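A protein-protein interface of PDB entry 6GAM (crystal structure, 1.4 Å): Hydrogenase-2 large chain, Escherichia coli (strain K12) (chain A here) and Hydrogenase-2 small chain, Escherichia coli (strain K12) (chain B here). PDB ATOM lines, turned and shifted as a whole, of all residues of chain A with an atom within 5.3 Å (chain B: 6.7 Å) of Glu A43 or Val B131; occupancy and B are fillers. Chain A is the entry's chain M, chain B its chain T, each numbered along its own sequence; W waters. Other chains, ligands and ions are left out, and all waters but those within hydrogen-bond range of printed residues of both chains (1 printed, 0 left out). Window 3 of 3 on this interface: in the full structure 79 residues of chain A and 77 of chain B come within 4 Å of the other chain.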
ATOM      1  N   TRP A  38       7.626 -25.866  27.888  1.00  0.00           N
ATOM      2  CA  TRP A  38       6.658 -25.469  26.872  1.00  0.00           C
ATOM      3  C   TRP A  38       6.195 -24.044  27.069  1.00  0.00           C
ATOM      4  O   TRP A  38       6.048 -23.566  28.210  1.00  0.00           O
ATOM      5  CB  TRP A  38       5.473 -26.446  26.878  1.00  0.00           C
ATOM      6  CG  TRP A  38       4.359 -26.152  25.900  1.00  0.00           C
ATOM      7  CD1 TRP A  38       4.375 -26.326  24.552  1.00  0.00           C
ATOM      8  CD2 TRP A  38       3.024 -25.752  26.228  1.00  0.00           C
ATOM      9  NE1 TRP A  38       3.165 -26.007  24.007  1.00  0.00           N
ATOM     10  CE2 TRP A  38       2.298 -25.694  25.025  1.00  0.00           C
ATOM     11  CE3 TRP A  38       2.356 -25.466  27.432  1.00  0.00           C
ATOM     12  CZ2 TRP A  38       0.976 -25.334  24.976  1.00  0.00           C
ATOM     13  CZ3 TRP A  38       1.054 -25.061  27.370  1.00  0.00           C
ATOM     14  CH2 TRP A  38       0.356 -25.025  26.134  1.00  0.00           C
ATOM     15  N   GLY A  40       3.714 -22.691  24.350  1.00  0.00           N
ATOM     16  CA  GLY A  40       2.447 -22.515  23.647  1.00  0.00           C
ATOM     17  C   GLY A  40       2.453 -21.423  22.589  1.00  0.00           C
ATOM     18  O   GLY A  40       1.530 -20.663  22.458  1.00  0.00           O
ATOM     19  N   MET A  41       3.566 -21.376  21.846  1.00  0.00           N
ATOM     20  CA  MET A  41       3.743 -20.319  20.823  1.00  0.00           C
ATOM     21  C   MET A  41       2.690 -20.431  19.719  1.00  0.00           C
ATOM     22  O   MET A  41       2.253 -19.442  19.175  1.00  0.00           O
ATOM     23  CB  MET A  41       5.136 -20.384  20.243  1.00  0.00           C
ATOM     24  CG  MET A  41       6.237 -20.166  21.264  1.00  0.00           C
ATOM     25  SD  MET A  41       6.274 -18.541  22.055  1.00  0.00           S
ATOM     26  CE  MET A  41       6.966 -17.517  20.767  1.00  0.00           C
ATOM     27  N   GLU A  42       2.305 -21.660  19.386  1.00  0.00           N
ATOM     28  CA  GLU A  42       1.224 -21.846  18.412  1.00  0.00           C
ATOM     29  C   GLU A  42      -0.098 -21.225  18.838  1.00  0.00           C
ATOM     30  O   GLU A  42      -0.839 -20.686  18.022  1.00  0.00           O
ATOM     31  CB  GLU A  42       1.062 -23.344  18.113  1.00  0.00           C
ATOM     32  CG  GLU A  42       2.265 -23.935  17.365  1.00  0.00           C
ATOM     33  CD  GLU A  42       2.456 -25.452  17.535  1.00  0.00           C
ATOM     34  OE1 GLU A  42       1.987 -25.970  18.600  1.00  0.00           O
ATOM     35  OE2 GLU A  42       3.128 -26.119  16.686  1.00  0.00           O
ATOM     36  N   GLU A  43      -0.428 -21.328  20.098  1.00  0.00           N
ATOM     37  CA  GLU A  43      -1.648 -20.728  20.670  1.00  0.00           C
ATOM     38  C   GLU A  43      -1.516 -19.203  20.764  1.00  0.00           C
ATOM     39  O   GLU A  43      -2.445 -18.495  20.459  1.00  0.00           O
ATOM     40  CB  GLU A  43      -1.971 -21.354  22.042  1.00  0.00           C
ATOM     41  CG  GLU A  43      -3.255 -20.876  22.720  1.00  0.00           C
ATOM     42  CD  GLU A  43      -3.685 -21.767  23.911  1.00  0.00           C
ATOM     43  OE1 GLU A  43      -2.894 -22.657  24.360  1.00  0.00           O
ATOM     44  OE2 GLU A  43      -4.832 -21.610  24.421  1.00  0.00           O
ATOM     45  N   ILE A  44      -0.332 -18.705  21.159  1.00  0.00           N
ATOM     46  CA  ILE A  44      -0.114 -17.262  21.266  1.00  0.00           C
ATOM     47  C   ILE A  44      -0.376 -16.533  19.953  1.00  0.00           C
ATOM     48  O   ILE A  44      -0.924 -15.426  19.932  1.00  0.00           O
ATOM     49  CB  ILE A  44       1.316 -17.002  21.833  1.00  0.00           C
ATOM     50  CG1 ILE A  44       1.363 -17.434  23.305  1.00  0.00           C
ATOM     51  CG2 ILE A  44       1.677 -15.523  21.725  1.00  0.00           C
ATOM     52  CD1 ILE A  44       2.747 -17.532  23.895  1.00  0.00           C
ATOM     53  N   VAL A  45      -0.014 -17.138  18.825  1.00  0.00           N
ATOM     54  CA  VAL A  45      -0.143 -16.489  17.564  1.00  0.00           C
ATOM     55  C   VAL A  45      -1.535 -16.619  16.942  1.00  0.00           C
ATOM     56  O   VAL A  45      -1.874 -15.940  15.987  1.00  0.00           O
ATOM     57  CB  VAL A  45       0.998 -16.993  16.612  1.00  0.00           C
ATOM     58  CG1 VAL A  45       0.669 -18.348  15.983  1.00  0.00           C
ATOM     59  CG2 VAL A  45       1.290 -15.952  15.551  1.00  0.00           C
ATOM     60  N   LYS A  46      -2.374 -17.514  17.477  1.00  0.00           N
ATOM     61  CA  LYS A  46      -3.730 -17.761  16.920  1.00  0.00           C
ATOM     62  C   LYS A  46      -4.602 -16.486  17.011  1.00  0.00           C
ATOM     63  O   LYS A  46      -4.457 -15.663  17.936  1.00  0.00           O
ATOM     64  CB  LYS A  46      -4.394 -18.912  17.703  1.00  0.00           C
ATOM     65  CG  LYS A  46      -5.648 -19.513  17.080  1.00  0.00           C
ATOM     66  CD  LYS A  46      -6.406 -20.454  18.077  1.00  0.00           C
ATOM     67  CE  LYS A  46      -7.830 -20.789  17.601  1.00  0.00           C
ATOM     68  NZ  LYS A  46      -8.765 -21.439  18.597  1.00  0.00           N
ATOM     69  N   THR A 349      -2.862 -28.502  19.912  1.00  0.00           N
ATOM     70  CA  THR A 349      -1.793 -28.482  20.930  1.00  0.00           C
ATOM     71  C   THR A 349      -2.398 -28.223  22.263  1.00  0.00           C
ATOM     72  O   THR A 349      -2.262 -27.142  22.837  1.00  0.00           O
ATOM     73  CB  THR A 349      -0.731 -27.414  20.585  1.00  0.00           C
ATOM     74  OG1 THR A 349      -0.361 -27.587  19.208  1.00  0.00           O
ATOM     75  CG2 THR A 349       0.481 -27.572  21.465  1.00  0.00           C
ATOM     76  N   PRO A 351      -2.512 -28.856  26.122  1.00  0.00           N
ATOM     77  CA  PRO A 351      -1.599 -29.425  27.110  1.00  0.00           C
ATOM     78  C   PRO A 351      -2.324 -30.394  28.050  1.00  0.00           C
ATOM     79  O   PRO A 351      -3.518 -30.190  28.349  1.00  0.00           O
ATOM     80  CB  PRO A 351      -1.072 -28.177  27.868  1.00  0.00           C
ATOM     81  CG  PRO A 351      -2.125 -27.179  27.705  1.00  0.00           C
ATOM     82  CD  PRO A 351      -2.683 -27.408  26.311  1.00  0.00           C
ATOM     83  N   ALA B 128       4.288 -14.557  27.564  1.00  0.00           N
ATOM     84  CA  ALA B 128       3.054 -14.184  28.310  1.00  0.00           C
ATOM     85  C   ALA B 128       1.956 -13.557  27.509  1.00  0.00           C
ATOM     86  O   ALA B 128       0.912 -13.144  28.056  1.00  0.00           O
ATOM     87  CB  ALA B 128       3.398 -13.263  29.473  1.00  0.00           C
ATOM     88  N   ALA B 129       2.140 -13.415  26.190  1.00  0.00           N
ATOM     89  CA  ALA B 129       1.202 -12.712  25.356  1.00  0.00           C
ATOM     90  C   ALA B 129      -0.023 -13.570  24.990  1.00  0.00           C
ATOM     91  O   ALA B 129      -0.089 -14.764  25.312  1.00  0.00           O
ATOM     92  CB  ALA B 129       1.899 -12.218  24.083  1.00  0.00           C
ATOM     93  N   GLY B 130      -0.966 -12.939  24.295  1.00  0.00           N
ATOM     94  CA  GLY B 130      -2.233 -13.592  23.957  1.00  0.00           C
ATOM     95  C   GLY B 130      -2.923 -14.176  25.209  1.00  0.00           C
ATOM     96  O   GLY B 130      -3.004 -13.566  26.263  1.00  0.00           O
ATOM     97  N   VAL B 131      -3.376 -15.404  25.087  1.00  0.00           N
ATOM     98  CA  VAL B 131      -4.037 -16.078  26.204  1.00  0.00           C
ATOM     99  C   VAL B 131      -3.102 -16.556  27.305  1.00  0.00           C
ATOM    100  O   VAL B 131      -3.548 -17.059  28.352  1.00  0.00           O
ATOM    101  CB  VAL B 131      -4.952 -17.236  25.697  1.00  0.00           C
ATOM    102  CG1 VAL B 131      -5.935 -16.710  24.642  1.00  0.00           C
ATOM    103  CG2 VAL B 131      -4.157 -18.411  25.160  1.00  0.00           C
ATOM    104  N   ASN B 132      -1.785 -16.419  27.108  1.00  0.00           N
ATOM    105  CA  ASN B 132      -0.800 -16.823  28.116  1.00  0.00           C
ATOM    106  C   ASN B 132      -1.029 -18.247  28.582  1.00  0.00           C
ATOM    107  O   ASN B 132      -1.362 -18.514  29.739  1.00  0.00           O
ATOM    108  CB  ASN B 132      -0.744 -15.830  29.299  1.00  0.00           C
ATOM    109  CG  ASN B 132       0.484 -16.029  30.193  1.00  0.00           C
ATOM    110  OD1 ASN B 132       1.273 -16.961  30.041  1.00  0.00           O
ATOM    111  ND2 ASN B 132       0.620 -15.169  31.191  1.00  0.00           N
ATOM    112  N   PRO B 133      -0.786 -19.206  27.692  1.00  0.00           N
ATOM    113  CA  PRO B 133      -1.051 -20.579  28.000  1.00  0.00           C
ATOM    114  C   PRO B 133      -0.438 -21.113  29.290  1.00  0.00           C
ATOM    115  O   PRO B 133      -0.980 -22.085  29.805  1.00  0.00           O
ATOM    116  CB  PRO B 133      -0.405 -21.343  26.839  1.00  0.00           C
ATOM    117  CG  PRO B 133      -0.379 -20.383  25.725  1.00  0.00           C
ATOM    118  CD  PRO B 133      -0.279 -19.015  26.309  1.00  0.00           C
ATOM    119  N   THR B 134       0.733 -20.629  29.731  1.00  0.00           N
ATOM    120  CA  THR B 134       1.442 -21.241  30.860  1.00  0.00           C
ATOM    121  C   THR B 134       1.448 -20.367  32.111  1.00  0.00           C
ATOM    122  O   THR B 134       2.155 -20.692  33.030  1.00  0.00           O
ATOM    123  CB  THR B 134       2.906 -21.558  30.492  1.00  0.00           C
ATOM    124  OG1 THR B 134       3.571 -20.324  30.155  1.00  0.00           O
ATOM    125  CG2 THR B 134       2.986 -22.528  29.306  1.00  0.00           C
ATOM    126  N   GLY B 135       0.673 -19.292  32.127  1.00  0.00           N
ATOM    127  CA  GLY B 135       0.699 -18.360  33.276  1.00  0.00           C
ATOM    128  C   GLY B 135       2.095 -17.798  33.511  1.00  0.00           C
ATOM    129  O   GLY B 135       2.582 -17.703  34.645  1.00  0.00           O
HETATM  130  O   HOH W   1      -3.506 -16.423  22.249  1.00  0.00           O
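Of the printed residues of chain B, Trp A38 touches Pro B133 (3.8 Å) and Thr B134 (3.4 Å).
Of the printed residues of chain B, Gly A40 touches Pro B133.
Of the printed residues of chain B, Ile A44 touches Ala B129 and Pro B133.
Of the printed residues of chain A, Ala B129 touches Ile A44 (3.6 Å).
Val B131 touches just one residue of chain A: Glu A43.
Asn B132 touches none of the printed residues of chain A.
Printed residues of chain A within 4 Å of Thr B134: Trp A38 (3.4 Å).
The nearest residue of chain B that does not touch Glu A43 is Gly B130 (6.0 Å).
The nearest printed residue of chain A that does not touch Val B131 is Ile A44 (5.4 Å).
The nearest printed residue of chain B that does not touch Ile A44 is Gly B130 (4.5 Å).
Water W1 lies within hydrogen-bond range of the backbone carbonyl oxygen of Glu A43 (2.9 Å) and the backbone NH of Val B131 (3.0 Å).
Among the printed residues, merely in contact across the chains: Trp A38 with Pro B133, Trp A38 with Thr B134, Gly A40 with Pro B133, Glu A43 with Val B131, Glu A43 with Pro B133, Ile A44 with Ala B129 and Ile A44 with Pro B133.
Printed residues of chain B that touch a printed residue of chain A: Ala B129, Val B131, Pro B133 and Thr B134.
Hydrophobic or aromatic side chains of chain B within 4 Å of the printed part of chain A: Val B131 and Pro B133.
Hydrophobic or aromatic side chains of chain A within 4 Å of the printed part of chain B: Trp A38 and Ile A44.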
